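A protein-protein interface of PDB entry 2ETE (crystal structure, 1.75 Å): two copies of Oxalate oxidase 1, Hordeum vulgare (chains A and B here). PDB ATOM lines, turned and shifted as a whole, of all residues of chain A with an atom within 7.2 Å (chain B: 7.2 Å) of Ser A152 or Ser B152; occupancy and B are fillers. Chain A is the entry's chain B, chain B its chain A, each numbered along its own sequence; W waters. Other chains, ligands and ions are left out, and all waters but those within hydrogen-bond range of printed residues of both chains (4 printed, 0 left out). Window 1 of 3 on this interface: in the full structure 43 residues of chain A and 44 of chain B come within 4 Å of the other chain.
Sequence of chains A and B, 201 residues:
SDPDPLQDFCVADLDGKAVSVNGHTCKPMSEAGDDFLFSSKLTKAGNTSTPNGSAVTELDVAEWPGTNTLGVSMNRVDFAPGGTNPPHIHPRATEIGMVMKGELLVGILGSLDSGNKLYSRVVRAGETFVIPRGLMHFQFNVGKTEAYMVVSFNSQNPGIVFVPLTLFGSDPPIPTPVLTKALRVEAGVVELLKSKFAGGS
The side-chain hydroxyl (OG) of Ser A152 sits at hydrogen-bond distance from the side-chain hydroxyl (OG) of Ser B152, at 3.4 Å.
Among the printed residues, merely in contact across the chains: Ile A96 with Met B74, Val A72 with Thr B94, Thr A94 with Val B72, Met A74 with Ile B96, Val A150 with Met B98, Ser A73 with Ile B96, Val A72 with Ile B96, Met A98 with Val B150, Ile A96 with Ser B73, Ser A152 with Ile B96, Ile A96 with Val B72, Asn A154 with Asn B154, Ile A96 with Ser B152, Val A72 with Asn B154 and Asn A154 with Val B72.
Water W4 lies within hydrogen-bond range of OG of Ser A152 (2.7 Å), O of Ile B96 (2.9 Å) and OG of Ser B152 (3.0 Å).
Water W1 lies within hydrogen-bond range of the backbone carbonyl oxygen of Ile A96, the side-chain hydroxyl of Ser B152 and the side-chain hydroxyl of Ser A152.
Water W3 bridges O of Asn A154 and ND2 of Asn B154.
Water W2 bridges O of Asn B154 (3.0 Å) and ND2 of Asn A154 (3.1 Å).
Ser A152 touches two residues of chain B.
Of the printed residues of chain B, Ser A73 touches Ile B96 (3.8 Å).
Of the printed residues of chain B, Asn A154 touches Val B72 and Asn B154.
The nearest residue of chain B that does not touch Ser A152 is Val B72 (5.6 Å).
Val A72 touches Ile B96, and with the chains exchanged Ile A96 touches Val B72.
Val A72 touches Asn B154, and with the chains exchanged Asn A154 touches Val B72.
Ile A96 touches Ser B152, and with the chains exchanged Ser A152 touches Ile B96.
Met A98 touches Val B150, and with the chains exchanged Val A150 touches Met B98.
17 positions are printed for both chains.
Of the 16 pairs that touch across the chains among the printed residues, 16 have their exchanged pair printed and touching as well.
Printed residues of chain A that touch a printed residue of chain B: Val A72, Ser A73, Met A74, Thr A94, Ile A96, Met A98, Val A150, Ser A152 and Asn A154.
Of the 17 printed residues of chain B, 9 touch a printed residue of chain A.
Hydrophobic or aromatic side chains of chain B within 4 Å of the printed part of chain A: Val B72, Met B74, Ile B96, Met B98 and Val B150.
Among the printed residues, no Asp or Glu carboxylate lies within 4 Å of a Lys or Arg side-chain nitrogen of the other chain.
The backbone NH (N) of Phe B153 lies within hydrogen-bond range of the backbone carbonyl oxygen (O) of Ser B73 (3.0 Å).
The side-chain hydroxyl (OG) of Ser B73 is in hydrogen-bond range of the backbone carbonyl oxygen (O) of Ser B155.
The backbone carbonyl oxygen (O) of Ile B96 lies within hydrogen-bond range of the backbone NH (N) of Ser B152, 2.8 Å away.
OG of Ser A73 is in hydrogen-bond range of O of Ser A155 (2.7 Å).
The backbone NH of Thr A94 sits at hydrogen-bond distance from the side-chain amide oxygen of Asn A154, 2.9 Å away.
The backbone carbonyl oxygen of Met A98 sits at hydrogen-bond distance from the backbone NH of Val A150 (3.0 Å).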
ATOM      1  N   VAL A  72      -3.202   8.679 -32.123  1.00  0.00           N
ATOM      2  CA  VAL A  72      -2.582   7.678 -31.246  1.00  0.00           C
ATOM      3  C   VAL A  72      -1.379   7.006 -31.915  1.00  0.00           C
ATOM      4  O   VAL A  72      -1.245   7.032 -33.143  1.00  0.00           O
ATOM      5  CB  VAL A  72      -3.579   6.556 -30.827  1.00  0.00           C
ATOM      6  CG1 VAL A  72      -4.667   7.081 -29.883  1.00  0.00           C
ATOM      7  CG2 VAL A  72      -4.194   5.889 -32.066  1.00  0.00           C
ATOM      8  N   SER A  73      -0.509   6.429 -31.088  1.00  0.00           N
ATOM      9  CA  SER A  73       0.568   5.536 -31.537  1.00  0.00           C
ATOM     10  C   SER A  73       1.077   4.724 -30.345  1.00  0.00           C
ATOM     11  O   SER A  73       0.631   4.923 -29.205  1.00  0.00           O
ATOM     12  CB  SER A  73       1.717   6.312 -32.203  1.00  0.00           C
ATOM     13  OG  SER A  73       2.395   7.142 -31.273  1.00  0.00           O
ATOM     14  N   MET A  74       2.015   3.819 -30.608  1.00  0.00           N
ATOM     15  CA  MET A  74       2.570   2.960 -29.567  1.00  0.00           C
ATOM     16  C   MET A  74       4.071   2.792 -29.745  1.00  0.00           C
ATOM     17  O   MET A  74       4.622   3.112 -30.804  1.00  0.00           O
ATOM     18  CB  MET A  74       1.930   1.571 -29.623  1.00  0.00           C
ATOM     19  CG  MET A  74       0.481   1.491 -29.209  1.00  0.00           C
ATOM     20  SD  MET A  74      -0.130  -0.197 -29.420  1.00  0.00           S
ATOM     21  CE  MET A  74       0.634  -1.004 -28.038  1.00  0.00           C
ATOM     22  N   ASN A  75       4.731   2.312 -28.697  1.00  0.00           N
ATOM     23  CA  ASN A  75       6.021   1.645 -28.866  1.00  0.00           C
ATOM     24  C   ASN A  75       6.314   0.606 -27.789  1.00  0.00           C
ATOM     25  O   ASN A  75       5.603   0.510 -26.786  1.00  0.00           O
ATOM     26  CB  ASN A  75       7.193   2.623 -29.099  1.00  0.00           C
ATOM     27  CG  ASN A  75       7.575   3.436 -27.878  1.00  0.00           C
ATOM     28  OD1 ASN A  75       7.929   4.614 -28.014  1.00  0.00           O
ATOM     29  ND2 ASN A  75       7.564   2.825 -26.701  1.00  0.00           N
ATOM     30  N   ALA A  93       3.028  14.818 -26.968  1.00  0.00           N
ATOM     31  CA  ALA A  93       2.117  13.787 -26.444  1.00  0.00           C
ATOM     32  C   ALA A  93       2.316  13.459 -24.971  1.00  0.00           C
ATOM     33  O   ALA A  93       3.446  13.495 -24.468  1.00  0.00           O
ATOM     34  CB  ALA A  93       2.246  12.508 -27.263  1.00  0.00           C
ATOM     35  N   THR A  94       1.221  13.134 -24.282  1.00  0.00           N
ATOM     36  CA  THR A  94       1.361  12.364 -23.042  1.00  0.00           C
ATOM     37  C   THR A  94       1.458  10.869 -23.341  1.00  0.00           C
ATOM     38  O   THR A  94       0.956  10.384 -24.369  1.00  0.00           O
ATOM     39  CB  THR A  94       0.388  12.761 -21.851  1.00  0.00           C
ATOM     40  OG1 THR A  94      -0.332  11.624 -21.341  1.00  0.00           O
ATOM     41  CG2 THR A  94      -0.530  13.868 -22.196  1.00  0.00           C
ATOM     42  N   GLU A  95       2.178  10.175 -22.464  1.00  0.00           N
ATOM     43  CA  GLU A  95       2.482   8.758 -22.606  1.00  0.00           C
ATOM     44  C   GLU A  95       1.772   7.996 -21.499  1.00  0.00           C
ATOM     45  O   GLU A  95       1.709   8.465 -20.360  1.00  0.00           O
ATOM     46  CB  GLU A  95       3.998   8.558 -22.483  1.00  0.00           C
ATOM     47  CG  GLU A  95       4.486   7.106 -22.510  1.00  0.00           C
ATOM     48  CD  GLU A  95       5.998   7.006 -22.376  1.00  0.00           C
ATOM     49  OE1 GLU A  95       6.684   8.017 -22.602  1.00  0.00           O
ATOM     50  OE2 GLU A  95       6.505   5.915 -22.047  1.00  0.00           O
ATOM     51  N   ILE A  96       1.249   6.822 -21.839  1.00  0.00           N
ATOM     52  CA  ILE A  96       0.617   5.942 -20.861  1.00  0.00           C
ATOM     53  C   ILE A  96       1.093   4.506 -21.118  1.00  0.00           C
ATOM     54  O   ILE A  96       0.997   3.995 -22.235  1.00  0.00           O
ATOM     55  CB  ILE A  96      -0.943   6.099 -20.856  1.00  0.00           C
ATOM     56  CG1 ILE A  96      -1.563   5.408 -19.633  1.00  0.00           C
ATOM     57  CG2 ILE A  96      -1.574   5.634 -22.184  1.00  0.00           C
ATOM     58  CD1 ILE A  96      -2.999   5.838 -19.353  1.00  0.00           C
ATOM     59  N   GLY A  97       1.640   3.873 -20.088  1.00  0.00           N
ATOM     60  CA  GLY A  97       2.348   2.613 -20.289  1.00  0.00           C
ATOM     61  C   GLY A  97       2.125   1.528 -19.260  1.00  0.00           C
ATOM     62  O   GLY A  97       1.656   1.789 -18.151  1.00  0.00           O
ATOM     63  N   MET A  98       2.475   0.303 -19.643  1.00  0.00           N
ATOM     64  CA  MET A  98       2.408  -0.851 -18.750  1.00  0.00           C
ATOM     65  C   MET A  98       3.712  -1.645 -18.828  1.00  0.00           C
ATOM     66  O   MET A  98       4.198  -1.948 -19.922  1.00  0.00           O
ATOM     67  CB  MET A  98       1.223  -1.753 -19.122  1.00  0.00           C
ATOM     68  CG  MET A  98       1.117  -3.029 -18.287  1.00  0.00           C
ATOM     69  SD  MET A  98      -0.262  -4.103 -18.757  1.00  0.00           S
ATOM     70  CE  MET A  98      -1.628  -3.270 -17.956  1.00  0.00           C
ATOM     71  N   VAL A 150       5.256  -1.782 -22.734  1.00  0.00           N
ATOM     72  CA  VAL A 150       4.558  -1.357 -23.936  1.00  0.00           C
ATOM     73  C   VAL A 150       3.808  -0.078 -23.582  1.00  0.00           C
ATOM     74  O   VAL A 150       3.082  -0.037 -22.585  1.00  0.00           O
ATOM     75  CB  VAL A 150       3.596  -2.453 -24.453  1.00  0.00           C
ATOM     76  CG1 VAL A 150       2.797  -1.953 -25.638  1.00  0.00           C
ATOM     77  CG2 VAL A 150       4.377  -3.709 -24.846  1.00  0.00           C
ATOM     78  N   VAL A 151       4.012   0.968 -24.378  1.00  0.00           N
ATOM     79  CA  VAL A 151       3.420   2.273 -24.081  1.00  0.00           C
ATOM     80  C   VAL A 151       2.619   2.823 -25.263  1.00  0.00           C
ATOM     81  O   VAL A 151       2.856   2.450 -26.419  1.00  0.00           O
ATOM     82  CB  VAL A 151       4.478   3.316 -23.586  1.00  0.00           C
ATOM     83  CG1 VAL A 151       5.324   2.746 -22.439  1.00  0.00           C
ATOM     84  CG2 VAL A 151       5.377   3.788 -24.718  1.00  0.00           C
ATOM     85  N   SER A 152       1.666   3.698 -24.955  1.00  0.00           N
ATOM     86  CA  SER A 152       0.843   4.358 -25.954  1.00  0.00           C
ATOM     87  C   SER A 152       0.919   5.871 -25.761  1.00  0.00           C
ATOM     88  O   SER A 152       1.250   6.351 -24.669  1.00  0.00           O
ATOM     89  CB  SER A 152      -0.610   3.881 -25.851  1.00  0.00           C
ATOM     90  OG  SER A 152      -0.708   2.483 -26.074  1.00  0.00           O
ATOM     91  N   PHE A 153       0.623   6.613 -26.828  1.00  0.00           N
ATOM     92  CA  PHE A 153       0.682   8.073 -26.819  1.00  0.00           C
ATOM     93  C   PHE A 153      -0.592   8.630 -27.425  1.00  0.00           C
ATOM     94  O   PHE A 153      -1.212   7.986 -28.274  1.00  0.00           O
ATOM     95  CB  PHE A 153       1.862   8.576 -27.664  1.00  0.00           C
ATOM     96  CG  PHE A 153       3.204   8.031 -27.248  1.00  0.00           C
ATOM     97  CD1 PHE A 153       3.712   6.871 -27.829  1.00  0.00           C
ATOM     98  CD2 PHE A 153       3.967   8.692 -26.287  1.00  0.00           C
ATOM     99  CE1 PHE A 153       4.958   6.362 -27.445  1.00  0.00           C
ATOM    100  CE2 PHE A 153       5.217   8.198 -25.903  1.00  0.00           C
ATOM    101  CZ  PHE A 153       5.710   7.028 -26.482  1.00  0.00           C
ATOM    102  N   ASN A 154      -0.978   9.833 -27.002  1.00  0.00           N
ATOM    103  CA  ASN A 154      -2.092  10.525 -27.645  1.00  0.00           C
ATOM    104  C   ASN A 154      -1.627  11.394 -28.825  1.00  0.00           C
ATOM    105  O   ASN A 154      -2.147  12.485 -29.059  1.00  0.00           O
ATOM    106  CB  ASN A 154      -2.952  11.302 -26.624  1.00  0.00           C
ATOM    107  CG  ASN A 154      -2.228  12.493 -26.014  1.00  0.00           C
ATOM    108  OD1 ASN A 154      -1.002  12.596 -26.072  1.00  0.00           O
ATOM    109  ND2 ASN A 154      -2.994  13.399 -25.412  1.00  0.00           N
ATOM    110  N   SER A 155      -0.638  10.887 -29.563  1.00  0.00           N
ATOM    111  CA  SER A 155      -0.219  11.473 -30.845  1.00  0.00           C
ATOM    112  C   SER A 155       0.259  10.379 -31.788  1.00  0.00           C
ATOM    113  O   SER A 155       0.799   9.369 -31.340  1.00  0.00           O
ATOM    114  CB  SER A 155       0.911  12.494 -30.656  1.00  0.00           C
ATOM    115  OG  SER A 155       1.350  13.009 -31.915  1.00  0.00           O
ATOM    116  N   PRO A 158       4.675  11.418 -31.474  1.00  0.00           N
ATOM    117  CA  PRO A 158       4.977  12.140 -30.232  1.00  0.00           C
ATOM    118  C   PRO A 158       6.307  12.885 -30.263  1.00  0.00           C
ATOM    119  O   PRO A 158       6.424  13.948 -29.645  1.00  0.00           O
ATOM    120  CB  PRO A 158       5.025  11.033 -29.170  1.00  0.00           C
ATOM    121  CG  PRO A 158       5.169   9.766 -29.907  1.00  0.00           C
ATOM    122  CD  PRO A 158       4.543   9.965 -31.252  1.00  0.00           C
ATOM    123  N   VAL B  72      -5.538  10.777 -21.732  1.00  0.00           N
ATOM    124  CA  VAL B  72      -5.315   9.332 -21.889  1.00  0.00           C
ATOM    125  C   VAL B  72      -6.014   8.514 -20.794  1.00  0.00           C
ATOM    126  O   VAL B  72      -6.326   9.034 -19.718  1.00  0.00           O
ATOM    127  CB  VAL B  72      -3.796   8.971 -21.860  1.00  0.00           C
ATOM    128  CG1 VAL B  72      -3.071   9.506 -23.097  1.00  0.00           C
ATOM    129  CG2 VAL B  72      -3.137   9.480 -20.572  1.00  0.00           C
ATOM    130  N   SER B  73      -6.253   7.236 -21.090  1.00  0.00           N
ATOM    131  CA  SER B  73      -6.708   6.249 -20.103  1.00  0.00           C
ATOM    132  C   SER B  73      -6.451   4.845 -20.656  1.00  0.00           C
ATOM    133  O   SER B  73      -6.009   4.692 -21.799  1.00  0.00           O
ATOM    134  CB  SER B  73      -8.190   6.439 -19.737  1.00  0.00           C
ATOM    135  OG  SER B  73      -9.042   6.168 -20.839  1.00  0.00           O
ATOM    136  N   MET B  74      -6.708   3.827 -19.842  1.00  0.00           N
ATOM    137  CA  MET B  74      -6.488   2.442 -20.262  1.00  0.00           C
ATOM    138  C   MET B  74      -7.611   1.548 -19.776  1.00  0.00           C
ATOM    139  O   MET B  74      -8.376   1.927 -18.890  1.00  0.00           O
ATOM    140  CB  MET B  74      -5.179   1.908 -19.677  1.00  0.00           C
ATOM    141  CG  MET B  74      -3.921   2.495 -20.243  1.00  0.00           C
ATOM    142  SD  MET B  74      -2.487   1.883 -19.326  1.00  0.00           S
ATOM    143  CE  MET B  74      -2.349   0.228 -19.962  1.00  0.00           C
ATOM    144  N   ASN B  75      -7.725   0.369 -20.378  1.00  0.00           N
ATOM    145  CA  ASN B  75      -8.344  -0.756 -19.682  1.00  0.00           C
ATOM    146  C   ASN B  75      -7.823  -2.116 -20.098  1.00  0.00           C
ATOM    147  O   ASN B  75      -7.071  -2.241 -21.070  1.00  0.00           O
ATOM    148  CB  ASN B  75      -9.883  -0.705 -19.664  1.00  0.00           C
ATOM    149  CG  ASN B  75     -10.519  -0.813 -21.029  1.00  0.00           C
ATOM    150  OD1 ASN B  75     -11.491  -0.103 -21.316  1.00  0.00           O
ATOM    151  ND2 ASN B  75     -10.025  -1.722 -21.861  1.00  0.00           N
ATOM    152  N   ALA B  93     -13.232   8.909 -28.116  1.00  0.00           N
ATOM    153  CA  ALA B  93     -11.826   8.493 -28.194  1.00  0.00           C
ATOM    154  C   ALA B  93     -11.527   7.468 -29.272  1.00  0.00           C
ATOM    155  O   ALA B  93     -12.362   6.614 -29.575  1.00  0.00           O
ATOM    156  CB  ALA B  93     -11.352   7.949 -26.843  1.00  0.00           C
ATOM    157  N   THR B  94     -10.317   7.575 -29.822  1.00  0.00           N
ATOM    158  CA  THR B  94      -9.672   6.501 -30.577  1.00  0.00           C
ATOM    159  C   THR B  94      -9.096   5.500 -29.575  1.00  0.00           C
ATOM    160  O   THR B  94      -8.625   5.891 -28.501  1.00  0.00           O
ATOM    161  CB  THR B  94      -8.538   7.063 -31.472  1.00  0.00           C
ATOM    162  OG1 THR B  94      -9.096   7.956 -32.444  1.00  0.00           O
ATOM    163  CG2 THR B  94      -7.784   5.940 -32.201  1.00  0.00           C
ATOM    164  N   GLU B  95      -9.162   4.213 -29.921  1.00  0.00           N
ATOM    165  CA  GLU B  95      -8.614   3.127 -29.107  1.00  0.00           C
ATOM    166  C   GLU B  95      -7.417   2.490 -29.817  1.00  0.00           C
ATOM    167  O   GLU B  95      -7.440   2.297 -31.034  1.00  0.00           O
ATOM    168  CB  GLU B  95      -9.692   2.060 -28.863  1.00  0.00           C
ATOM    169  CG  GLU B  95      -9.235   0.822 -28.079  1.00  0.00           C
ATOM    170  CD  GLU B  95     -10.347  -0.197 -27.885  1.00  0.00           C
ATOM    171  OE1 GLU B  95     -11.537   0.175 -27.984  1.00  0.00           O
ATOM    172  OE2 GLU B  95     -10.033  -1.380 -27.626  1.00  0.00           O
ATOM    173  N   ILE B  96      -6.379   2.171 -29.048  1.00  0.00           N
ATOM    174  CA  ILE B  96      -5.203   1.477 -29.582  1.00  0.00           C
ATOM    175  C   ILE B  96      -4.815   0.350 -28.616  1.00  0.00           C
ATOM    176  O   ILE B  96      -4.629   0.581 -27.421  1.00  0.00           O
ATOM    177  CB  ILE B  96      -4.038   2.474 -29.894  1.00  0.00           C
ATOM    178  CG1 ILE B  96      -2.943   1.812 -30.740  1.00  0.00           C
ATOM    179  CG2 ILE B  96      -3.471   3.122 -28.616  1.00  0.00           C
ATOM    180  CD1 ILE B  96      -2.056   2.813 -31.471  1.00  0.00           C
ATOM    181  N   GLY B  97      -4.725  -0.876 -29.129  1.00  0.00           N
ATOM    182  CA  GLY B  97      -4.606  -2.025 -28.239  1.00  0.00           C
ATOM    183  C   GLY B  97      -3.623  -3.101 -28.640  1.00  0.00           C
ATOM    184  O   GLY B  97      -3.220  -3.183 -29.799  1.00  0.00           O
ATOM    185  N   MET B  98      -3.248  -3.921 -27.661  1.00  0.00           N
ATOM    186  CA  MET B  98      -2.390  -5.086 -27.878  1.00  0.00           C
ATOM    187  C   MET B  98      -3.000  -6.321 -27.216  1.00  0.00           C
ATOM    188  O   MET B  98      -3.417  -6.273 -26.059  1.00  0.00           O
ATOM    189  CB  MET B  98      -0.982  -4.836 -27.320  1.00  0.00           C
ATOM    190  CG  MET B  98      -0.025  -6.030 -27.471  1.00  0.00           C
ATOM    191  SD  MET B  98       1.622  -5.737 -26.784  1.00  0.00           S
ATOM    192  CE  MET B  98       2.394  -4.794 -28.093  1.00  0.00           C
ATOM    193  N   VAL B 150      -4.816  -5.488 -23.492  1.00  0.00           N
ATOM    194  CA  VAL B 150      -4.679  -4.224 -22.789  1.00  0.00           C
ATOM    195  C   VAL B 150      -4.759  -3.117 -23.834  1.00  0.00           C
ATOM    196  O   VAL B 150      -4.020  -3.137 -24.825  1.00  0.00           O
ATOM    197  CB  VAL B 150      -3.345  -4.154 -22.017  1.00  0.00           C
ATOM    198  CG1 VAL B 150      -3.145  -2.775 -21.401  1.00  0.00           C
ATOM    199  CG2 VAL B 150      -3.302  -5.231 -20.930  1.00  0.00           C
ATOM    200  N   VAL B 151      -5.665  -2.166 -23.619  1.00  0.00           N
ATOM    201  CA  VAL B 151      -5.908  -1.109 -24.602  1.00  0.00           C
ATOM    202  C   VAL B 151      -5.780   0.279 -23.972  1.00  0.00           C
ATOM    203  O   VAL B 151      -5.964   0.446 -22.762  1.00  0.00           O
ATOM    204  CB  VAL B 151      -7.280  -1.271 -25.342  1.00  0.00           C
ATOM    205  CG1 VAL B 151      -7.440  -2.683 -25.931  1.00  0.00           C
ATOM    206  CG2 VAL B 151      -8.460  -0.956 -24.433  1.00  0.00           C
ATOM    207  N   SER B 152      -5.440   1.258 -24.803  1.00  0.00           N
ATOM    208  CA  SER B 152      -5.323   2.651 -24.375  1.00  0.00           C
ATOM    209  C   SER B 152      -6.232   3.530 -25.230  1.00  0.00           C
ATOM    210  O   SER B 152      -6.587   3.159 -26.353  1.00  0.00           O
ATOM    211  CB  SER B 152      -3.871   3.125 -24.478  1.00  0.00           C
ATOM    212  OG  SER B 152      -3.013   2.359 -23.643  1.00  0.00           O
ATOM    213  N   PHE B 153      -6.613   4.686 -24.688  1.00  0.00           N
ATOM    214  CA  PHE B 153      -7.472   5.645 -25.385  1.00  0.00           C
ATOM    215  C   PHE B 153      -6.849   7.033 -25.329  1.00  0.00           C
ATOM    216  O   PHE B 153      -6.117   7.348 -24.379  1.00  0.00           O
ATOM    217  CB  PHE B 153      -8.857   5.710 -24.721  1.00  0.00           C
ATOM    218  CG  PHE B 153      -9.539   4.376 -24.576  1.00  0.00           C
ATOM    219  CD1 PHE B 153      -9.355   3.603 -23.431  1.00  0.00           C
ATOM    220  CD2 PHE B 153     -10.376   3.898 -25.581  1.00  0.00           C
ATOM    221  CE1 PHE B 153      -9.990   2.361 -23.290  1.00  0.00           C
ATOM    222  CE2 PHE B 153     -11.016   2.666 -25.447  1.00  0.00           C
ATOM    223  CZ  PHE B 153     -10.820   1.898 -24.299  1.00  0.00           C
ATOM    224  N   ASN B 154      -7.144   7.862 -26.331  1.00  0.00           N
ATOM    225  CA  ASN B 154      -6.768   9.280 -26.284  1.00  0.00           C
ATOM    226  C   ASN B 154      -7.841  10.159 -25.611  1.00  0.00           C
ATOM    227  O   ASN B 154      -8.081  11.297 -26.017  1.00  0.00           O
ATOM    228  CB  ASN B 154      -6.344   9.813 -27.671  1.00  0.00           C
ATOM    229  CG  ASN B 154      -7.499   9.890 -28.669  1.00  0.00           C
ATOM    230  OD1 ASN B 154      -8.556   9.296 -28.471  1.00  0.00           O
ATOM    231  ND2 ASN B 154      -7.290  10.640 -29.755  1.00  0.00           N
ATOM    232  N   SER B 155      -8.470   9.607 -24.573  1.00  0.00           N
ATOM    233  CA  SER B 155      -9.347  10.363 -23.667  1.00  0.00           C
ATOM    234  C   SER B 155      -9.244   9.803 -22.252  1.00  0.00           C
ATOM    235  O   SER B 155      -9.030   8.603 -22.067  1.00  0.00           O
ATOM    236  CB  SER B 155     -10.813  10.292 -24.113  1.00  0.00           C
ATOM    237  OG  SER B 155     -11.657  11.001 -23.203  1.00  0.00           O
ATOM    238  N   PRO B 158     -13.311   7.795 -22.277  1.00  0.00           N
ATOM    239  CA  PRO B 158     -13.762   7.519 -23.648  1.00  0.00           C
ATOM    240  C   PRO B 158     -15.265   7.266 -23.784  1.00  0.00           C
ATOM    241  O   PRO B 158     -15.848   7.600 -24.821  1.00  0.00           O
ATOM    242  CB  PRO B 158     -12.972   6.261 -24.037  1.00  0.00           C
ATOM    243  CG  PRO B 158     -12.545   5.650 -22.751  1.00  0.00           C
ATOM    244  CD  PRO B 158     -12.332   6.794 -21.807  1.00  0.00           C
HETATM  245  O   HOH W   1      -0.296   1.733 -23.100  1.00  0.00           O
HETATM  246  O   HOH W   2      -5.909  13.272 -26.406  1.00  0.00           O
HETATM  247  O   HOH W   3      -5.034  12.767 -29.239  1.00  0.00           O
HETATM  248  O   HOH W   4      -2.321   0.318 -25.726  1.00  0.00           O
